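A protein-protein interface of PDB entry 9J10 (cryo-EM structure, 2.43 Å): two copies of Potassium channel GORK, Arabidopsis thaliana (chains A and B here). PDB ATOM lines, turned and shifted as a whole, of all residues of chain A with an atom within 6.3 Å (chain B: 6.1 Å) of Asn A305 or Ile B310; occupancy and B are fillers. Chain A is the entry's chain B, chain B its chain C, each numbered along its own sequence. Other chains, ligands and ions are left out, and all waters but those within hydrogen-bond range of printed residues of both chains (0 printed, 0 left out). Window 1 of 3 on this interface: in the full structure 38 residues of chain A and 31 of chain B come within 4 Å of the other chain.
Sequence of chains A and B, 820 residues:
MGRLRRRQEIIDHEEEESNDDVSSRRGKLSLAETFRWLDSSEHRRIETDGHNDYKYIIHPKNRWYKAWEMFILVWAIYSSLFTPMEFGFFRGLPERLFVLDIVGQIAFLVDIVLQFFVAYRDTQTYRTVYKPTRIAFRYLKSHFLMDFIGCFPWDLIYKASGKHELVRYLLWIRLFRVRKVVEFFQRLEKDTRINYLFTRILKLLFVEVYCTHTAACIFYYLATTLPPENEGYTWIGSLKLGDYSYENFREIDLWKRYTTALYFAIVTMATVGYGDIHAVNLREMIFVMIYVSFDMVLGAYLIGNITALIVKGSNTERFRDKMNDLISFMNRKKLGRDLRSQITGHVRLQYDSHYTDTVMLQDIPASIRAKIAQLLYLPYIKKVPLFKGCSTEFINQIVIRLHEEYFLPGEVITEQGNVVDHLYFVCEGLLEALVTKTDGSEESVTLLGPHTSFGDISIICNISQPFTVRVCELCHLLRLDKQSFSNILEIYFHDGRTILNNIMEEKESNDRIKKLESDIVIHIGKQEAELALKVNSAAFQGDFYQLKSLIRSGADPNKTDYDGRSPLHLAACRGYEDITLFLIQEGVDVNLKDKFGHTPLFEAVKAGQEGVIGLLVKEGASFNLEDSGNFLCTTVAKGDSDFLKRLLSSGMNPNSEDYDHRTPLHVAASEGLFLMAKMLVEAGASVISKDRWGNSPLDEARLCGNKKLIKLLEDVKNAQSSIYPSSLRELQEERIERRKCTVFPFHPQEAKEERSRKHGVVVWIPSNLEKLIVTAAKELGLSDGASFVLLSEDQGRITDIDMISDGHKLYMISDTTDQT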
ATOM      1  N   LEU A 197      13.441 -30.590  30.270  1.00  0.00           N
ATOM      2  CA  LEU A 197      14.412 -29.631  29.755  1.00  0.00           C
ATOM      3  C   LEU A 197      13.721 -28.427  29.133  1.00  0.00           C
ATOM      4  O   LEU A 197      14.256 -27.313  29.176  1.00  0.00           O
ATOM      5  CB  LEU A 197      15.333 -30.308  28.746  1.00  0.00           C
ATOM      6  CG  LEU A 197      16.658 -30.821  29.312  1.00  0.00           C
ATOM      7  CD1 LEU A 197      17.381 -31.675  28.287  1.00  0.00           C
ATOM      8  CD2 LEU A 197      17.535 -29.672  29.773  1.00  0.00           C
ATOM      9  N   ARG A 200      12.920 -26.144  31.869  1.00  0.00           N
ATOM     10  CA  ARG A 200      14.119 -25.449  32.318  1.00  0.00           C
ATOM     11  C   ARG A 200      14.483 -24.311  31.377  1.00  0.00           C
ATOM     12  O   ARG A 200      15.035 -23.295  31.816  1.00  0.00           O
ATOM     13  CB  ARG A 200      15.280 -26.431  32.439  1.00  0.00           C
ATOM     14  CG  ARG A 200      16.350 -26.009  33.421  1.00  0.00           C
ATOM     15  CD  ARG A 200      17.459 -27.040  33.496  1.00  0.00           C
ATOM     16  NE  ARG A 200      17.032 -28.244  34.201  1.00  0.00           N
ATOM     17  CZ  ARG A 200      17.864 -29.162  34.681  1.00  0.00           C
ATOM     18  NH1 ARG A 200      19.173 -29.009  34.536  1.00  0.00           N
ATOM     19  NH2 ARG A 200      17.388 -30.227  35.311  1.00  0.00           N
ATOM     20  N   ILE A 201      14.139 -24.437  30.094  1.00  0.00           N
ATOM     21  CA  ILE A 201      14.364 -23.339  29.160  1.00  0.00           C
ATOM     22  C   ILE A 201      13.367 -22.215  29.415  1.00  0.00           C
ATOM     23  O   ILE A 201      13.738 -21.034  29.445  1.00  0.00           O
ATOM     24  CB  ILE A 201      14.307 -23.858  27.710  1.00  0.00           C
ATOM     25  CG1 ILE A 201      15.583 -24.632  27.379  1.00  0.00           C
ATOM     26  CG2 ILE A 201      14.105 -22.731  26.710  1.00  0.00           C
ATOM     27  CD1 ILE A 201      15.382 -25.751  26.388  1.00  0.00           C
ATOM     28  N   LEU A 204      14.310 -20.382  32.520  1.00  0.00           N
ATOM     29  CA  LEU A 204      15.432 -19.482  32.301  1.00  0.00           C
ATOM     30  C   LEU A 204      15.032 -18.271  31.467  1.00  0.00           C
ATOM     31  O   LEU A 204      15.624 -17.199  31.618  1.00  0.00           O
ATOM     32  CB  LEU A 204      16.572 -20.244  31.633  1.00  0.00           C
ATOM     33  CG  LEU A 204      17.925 -19.559  31.523  1.00  0.00           C
ATOM     34  CD1 LEU A 204      18.466 -19.285  32.904  1.00  0.00           C
ATOM     35  CD2 LEU A 204      18.857 -20.453  30.771  1.00  0.00           C
ATOM     36  N   ALA A 300      25.332 -17.546  27.848  1.00  0.00           N
ATOM     37  CA  ALA A 300      26.006 -18.827  27.646  1.00  0.00           C
ATOM     38  C   ALA A 300      25.202 -19.980  28.234  1.00  0.00           C
ATOM     39  O   ALA A 300      25.137 -21.066  27.640  1.00  0.00           O
ATOM     40  CB  ALA A 300      27.405 -18.788  28.252  1.00  0.00           C
ATOM     41  N   TYR A 301      24.537 -19.744  29.369  1.00  0.00           N
ATOM     42  CA  TYR A 301      23.681 -20.767  29.966  1.00  0.00           C
ATOM     43  C   TYR A 301      22.482 -21.088  29.081  1.00  0.00           C
ATOM     44  O   TYR A 301      22.106 -22.260  28.937  1.00  0.00           O
ATOM     45  CB  TYR A 301      23.216 -20.305  31.343  1.00  0.00           C
ATOM     46  CG  TYR A 301      22.951 -21.424  32.312  1.00  0.00           C
ATOM     47  CD1 TYR A 301      23.993 -22.143  32.876  1.00  0.00           C
ATOM     48  CD2 TYR A 301      21.654 -21.757  32.672  1.00  0.00           C
ATOM     49  CE1 TYR A 301      23.750 -23.171  33.766  1.00  0.00           C
ATOM     50  CE2 TYR A 301      21.399 -22.779  33.560  1.00  0.00           C
ATOM     51  CZ  TYR A 301      22.450 -23.483  34.103  1.00  0.00           C
ATOM     52  OH  TYR A 301      22.198 -24.503  34.990  1.00  0.00           O
ATOM     53  N   LEU A 302      21.891 -20.061  28.460  1.00  0.00           N
ATOM     54  CA  LEU A 302      20.748 -20.286  27.574  1.00  0.00           C
ATOM     55  C   LEU A 302      21.139 -21.096  26.338  1.00  0.00           C
ATOM     56  O   LEU A 302      20.429 -22.039  25.947  1.00  0.00           O
ATOM     57  CB  LEU A 302      20.136 -18.949  27.166  1.00  0.00           C
ATOM     58  CG  LEU A 302      19.145 -19.007  26.006  1.00  0.00           C
ATOM     59  CD1 LEU A 302      17.807 -19.509  26.493  1.00  0.00           C
ATOM     60  CD2 LEU A 302      19.001 -17.657  25.344  1.00  0.00           C
ATOM     61  N   ILE A 303      22.280 -20.751  25.725  1.00  0.00           N
ATOM     62  CA  ILE A 303      22.756 -21.479  24.547  1.00  0.00           C
ATOM     63  C   ILE A 303      23.062 -22.932  24.893  1.00  0.00           C
ATOM     64  O   ILE A 303      22.691 -23.853  24.149  1.00  0.00           O
ATOM     65  CB  ILE A 303      23.977 -20.762  23.941  1.00  0.00           C
ATOM     66  CG1 ILE A 303      23.543 -19.503  23.203  1.00  0.00           C
ATOM     67  CG2 ILE A 303      24.726 -21.649  22.974  1.00  0.00           C
ATOM     68  CD1 ILE A 303      24.691 -18.624  22.805  1.00  0.00           C
ATOM     69  N   GLY A 304      23.689 -23.162  26.055  1.00  0.00           N
ATOM     70  CA  GLY A 304      23.993 -24.523  26.468  1.00  0.00           C
ATOM     71  C   GLY A 304      22.758 -25.364  26.730  1.00  0.00           C
ATOM     72  O   GLY A 304      22.725 -26.548  26.389  1.00  0.00           O
ATOM     73  N   ASN A 305      21.713 -24.754  27.295  1.00  0.00           N
ATOM     74  CA  ASN A 305      20.482 -25.500  27.547  1.00  0.00           C
ATOM     75  C   ASN A 305      19.768 -25.877  26.256  1.00  0.00           C
ATOM     76  O   ASN A 305      19.264 -27.001  26.129  1.00  0.00           O
ATOM     77  CB  ASN A 305      19.555 -24.695  28.445  1.00  0.00           C
ATOM     78  CG  ASN A 305      19.621 -25.138  29.875  1.00  0.00           C
ATOM     79  OD1 ASN A 305      19.452 -26.315  30.175  1.00  0.00           O
ATOM     80  ND2 ASN A 305      19.884 -24.204  30.772  1.00  0.00           N
ATOM     81  N   ILE A 306      19.731 -24.965  25.281  1.00  0.00           N
ATOM     82  CA  ILE A 306      19.072 -25.284  24.015  1.00  0.00           C
ATOM     83  C   ILE A 306      19.847 -26.362  23.256  1.00  0.00           C
ATOM     84  O   ILE A 306      19.253 -27.289  22.681  1.00  0.00           O
ATOM     85  CB  ILE A 306      18.882 -23.997  23.193  1.00  0.00           C
ATOM     86  CG1 ILE A 306      17.720 -23.196  23.774  1.00  0.00           C
ATOM     87  CG2 ILE A 306      18.617 -24.286  21.732  1.00  0.00           C
ATOM     88  CD1 ILE A 306      17.448 -21.909  23.062  1.00  0.00           C
ATOM     89  N   THR A 307      21.183 -26.305  23.313  1.00  0.00           N
ATOM     90  CA  THR A 307      22.003 -27.327  22.666  1.00  0.00           C
ATOM     91  C   THR A 307      21.817 -28.694  23.317  1.00  0.00           C
ATOM     92  O   THR A 307      21.677 -29.703  22.616  1.00  0.00           O
ATOM     93  CB  THR A 307      23.471 -26.915  22.702  1.00  0.00           C
ATOM     94  OG1 THR A 307      23.620 -25.644  22.064  1.00  0.00           O
ATOM     95  CG2 THR A 307      24.333 -27.925  21.977  1.00  0.00           C
ATOM     96  N   ALA A 308      21.764 -28.740  24.653  1.00  0.00           N
ATOM     97  CA  ALA A 308      21.546 -30.008  25.340  1.00  0.00           C
ATOM     98  C   ALA A 308      20.146 -30.554  25.104  1.00  0.00           C
ATOM     99  O   ALA A 308      19.935 -31.767  25.203  1.00  0.00           O
ATOM    100  CB  ALA A 308      21.785 -29.848  26.836  1.00  0.00           C
ATOM    101  N   LEU A 309      19.180 -29.686  24.807  1.00  0.00           N
ATOM    102  CA  LEU A 309      17.877 -30.187  24.387  1.00  0.00           C
ATOM    103  C   LEU A 309      17.947 -30.830  23.008  1.00  0.00           C
ATOM    104  O   LEU A 309      17.384 -31.909  22.793  1.00  0.00           O
ATOM    105  CB  LEU A 309      16.852 -29.060  24.392  1.00  0.00           C
ATOM    106  CG  LEU A 309      15.455 -29.495  23.960  1.00  0.00           C
ATOM    107  CD1 LEU A 309      14.815 -30.314  25.053  1.00  0.00           C
ATOM    108  CD2 LEU A 309      14.596 -28.302  23.609  1.00  0.00           C
ATOM    109  N   ILE A 310      18.635 -30.186  22.064  1.00  0.00           N
ATOM    110  CA  ILE A 310      18.598 -30.655  20.679  1.00  0.00           C
ATOM    111  C   ILE A 310      19.416 -31.937  20.507  1.00  0.00           C
ATOM    112  O   ILE A 310      18.999 -32.854  19.787  1.00  0.00           O
ATOM    113  CB  ILE A 310      19.060 -29.527  19.738  1.00  0.00           C
ATOM    114  CG1 ILE A 310      17.992 -28.446  19.675  1.00  0.00           C
ATOM    115  CG2 ILE A 310      19.280 -30.020  18.332  1.00  0.00           C
ATOM    116  CD1 ILE A 310      18.444 -27.198  18.984  1.00  0.00           C
ATOM    117  N   ASN B 305      32.509 -25.019  27.176  1.00  0.00           N
ATOM    118  CA  ASN B 305      32.635 -25.646  28.490  1.00  0.00           C
ATOM    119  C   ASN B 305      31.300 -25.713  29.221  1.00  0.00           C
ATOM    120  O   ASN B 305      30.986 -26.733  29.851  1.00  0.00           O
ATOM    121  CB  ASN B 305      33.657 -24.897  29.333  1.00  0.00           C
ATOM    122  CG  ASN B 305      34.992 -25.578  29.345  1.00  0.00           C
ATOM    123  OD1 ASN B 305      35.089 -26.759  29.656  1.00  0.00           O
ATOM    124  ND2 ASN B 305      36.034 -24.846  28.990  1.00  0.00           N
ATOM    125  N   ILE B 306      30.493 -24.653  29.132  1.00  0.00           N
ATOM    126  CA  ILE B 306      29.192 -24.675  29.801  1.00  0.00           C
ATOM    127  C   ILE B 306      28.262 -25.695  29.144  1.00  0.00           C
ATOM    128  O   ILE B 306      27.539 -26.436  29.833  1.00  0.00           O
ATOM    129  CB  ILE B 306      28.599 -23.255  29.824  1.00  0.00           C
ATOM    130  CG1 ILE B 306      29.308 -22.430  30.894  1.00  0.00           C
ATOM    131  CG2 ILE B 306      27.109 -23.263  30.093  1.00  0.00           C
ATOM    132  CD1 ILE B 306      28.824 -21.019  31.000  1.00  0.00           C
ATOM    133  N   THR B 307      28.324 -25.807  27.812  1.00  0.00           N
ATOM    134  CA  THR B 307      27.513 -26.797  27.107  1.00  0.00           C
ATOM    135  C   THR B 307      27.925 -28.222  27.463  1.00  0.00           C
ATOM    136  O   THR B 307      27.064 -29.076  27.709  1.00  0.00           O
ATOM    137  CB  THR B 307      27.615 -26.575  25.601  1.00  0.00           C
ATOM    138  OG1 THR B 307      27.200 -25.241  25.292  1.00  0.00           O
ATOM    139  CG2 THR B 307      26.729 -27.544  24.850  1.00  0.00           C
ATOM    140  N   ALA B 308      29.233 -28.484  27.546  1.00  0.00           N
ATOM    141  CA  ALA B 308      29.698 -29.815  27.924  1.00  0.00           C
ATOM    142  C   ALA B 308      29.377 -30.144  29.373  1.00  0.00           C
ATOM    143  O   ALA B 308      29.270 -31.321  29.727  1.00  0.00           O
ATOM    144  CB  ALA B 308      31.200 -29.936  27.694  1.00  0.00           C
ATOM    145  N   LEU B 309      29.232 -29.130  30.224  1.00  0.00           N
ATOM    146  CA  LEU B 309      28.737 -29.394  31.570  1.00  0.00           C
ATOM    147  C   LEU B 309      27.268 -29.801  31.551  1.00  0.00           C
ATOM    148  O   LEU B 309      26.876 -30.753  32.232  1.00  0.00           O
ATOM    149  CB  LEU B 309      28.932 -28.170  32.456  1.00  0.00           C
ATOM    150  CG  LEU B 309      28.435 -28.358  33.886  1.00  0.00           C
ATOM    151  CD1 LEU B 309      29.376 -29.267  34.637  1.00  0.00           C
ATOM    152  CD2 LEU B 309      28.292 -27.029  34.593  1.00  0.00           C
ATOM    153  N   ILE B 310      26.444 -29.094  30.775  1.00  0.00           N
ATOM    154  CA  ILE B 310      25.001 -29.317  30.841  1.00  0.00           C
ATOM    155  C   ILE B 310      24.613 -30.640  30.177  1.00  0.00           C
ATOM    156  O   ILE B 310      23.750 -31.368  30.686  1.00  0.00           O
ATOM    157  CB  ILE B 310      24.261 -28.111  30.233  1.00  0.00           C
ATOM    158  CG1 ILE B 310      24.384 -26.915  31.166  1.00  0.00           C
ATOM    159  CG2 ILE B 310      22.793 -28.383  30.048  1.00  0.00           C
ATOM    160  CD1 ILE B 310      23.911 -25.632  30.558  1.00  0.00           C
ATOM    161  N   VAL B 311      25.265 -30.989  29.061  1.00  0.00           N
ATOM    162  CA  VAL B 311      24.949 -32.210  28.310  1.00  0.00           C
ATOM    163  C   VAL B 311      25.156 -33.487  29.124  1.00  0.00           C
ATOM    164  O   VAL B 311      24.343 -34.415  29.035  1.00  0.00           O
ATOM    165  CB  VAL B 311      25.772 -32.213  27.003  1.00  0.00           C
ATOM    166  CG1 VAL B 311      25.763 -33.560  26.316  1.00  0.00           C
ATOM    167  CG2 VAL B 311      25.213 -31.194  26.041  1.00  0.00           C
ATOM    168  N   LYS B 312      26.148 -33.519  30.005  1.00  0.00           N
ATOM    169  CA  LYS B 312      26.416 -34.710  30.801  1.00  0.00           C
ATOM    170  C   LYS B 312      25.602 -34.674  32.092  1.00  0.00           C
ATOM    171  O   LYS B 312      26.163 -34.617  33.190  1.00  0.00           O
ATOM    172  CB  LYS B 312      27.890 -34.828  31.111  1.00  0.00           C
ATOM    173  CG  LYS B 312      28.140 -36.133  31.857  1.00  0.00           C
ATOM    174  CD  LYS B 312      29.633 -36.286  32.129  1.00  0.00           C
ATOM    175  CE  LYS B 312      29.883 -37.588  32.882  1.00  0.00           C
ATOM    176  NZ  LYS B 312      31.321 -37.735  33.144  1.00  0.00           N
ATOM    177  N   GLY B 313      24.276 -34.653  31.965  1.00  0.00           N
ATOM    178  CA  GLY B 313      23.397 -34.502  33.109  1.00  0.00           C
ATOM    179  C   GLY B 313      23.411 -35.680  34.072  1.00  0.00           C
ATOM    180  O   GLY B 313      24.081 -36.693  33.879  1.00  0.00           O
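The side-chain amide nitrogen (ND2) of Asn A305 lies within hydrogen-bond range of the backbone carbonyl oxygen (O) of Tyr A301 (3.5 Å). The backbone carbonyl oxygen (O) of Ile A303 lies within hydrogen-bond range of the side-chain hydroxyl (OG1) of Thr A307 (2.9 Å).
Among the printed residues, merely in contact across the chains: Gly A304 with Thr B307 (3.5 Å), Ala A308 with Ile B310 (3.7 Å), Thr A307 with Thr B307 (3.8 Å), Ala A308 with Val B311 (3.8 Å), Ala A300 with Ile B306 (3.8 Å) and Asn A305 with Ile B310 (3.9 Å).
Asn A305 touches just one residue of chain B: Ile B310. Printed residues of chain A within 4 Å of Ile B310: Asn A305 (3.9 Å) and Ala A308 (3.7 Å). Of the printed residues of chain A, Val B311 touches Ala A308. Of the printed residues of chain B, Ala A308 touches Ile B310 (3.7 Å) and Val B311 (3.8 Å). Leu A302 touches none of the printed residues of chain B. The nearest residue of chain B that does not touch Asn A305 is Thr B307 (5.9 Å). The nearest printed residue of chain B that does not touch Gly A304 is Ile B310 (4.01 Å).
Printed residues of chain A that touch a printed residue of chain B: Ala A300, Gly A304, Asn A305, Thr A307 and Ala A308. Hydrophobic or aromatic side chains of chain B within 4 Å of the printed part of chain A: Ile B306, Ile B310 and Val B311. Along chain B the printed residues that touch a printed residue of chain A span positions 306 to 311. Among the printed residues, no Asp or Glu carboxylate lies within 4 Å of a Lys or Arg side-chain nitrogen of the other chain.
Asn A305 touches Ile B310, but with the chains exchanged Ile A310 does not touch Asn B305 (15.0 Å). Thr B307 touches its own counterpart, Thr A307. Ala A308 touches Ile B310, but with the chains exchanged Ile A310 does not touch Ala B308 (12.1 Å). Positions printed for both chains: 305, 306, 307, 308, 309 and 310.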
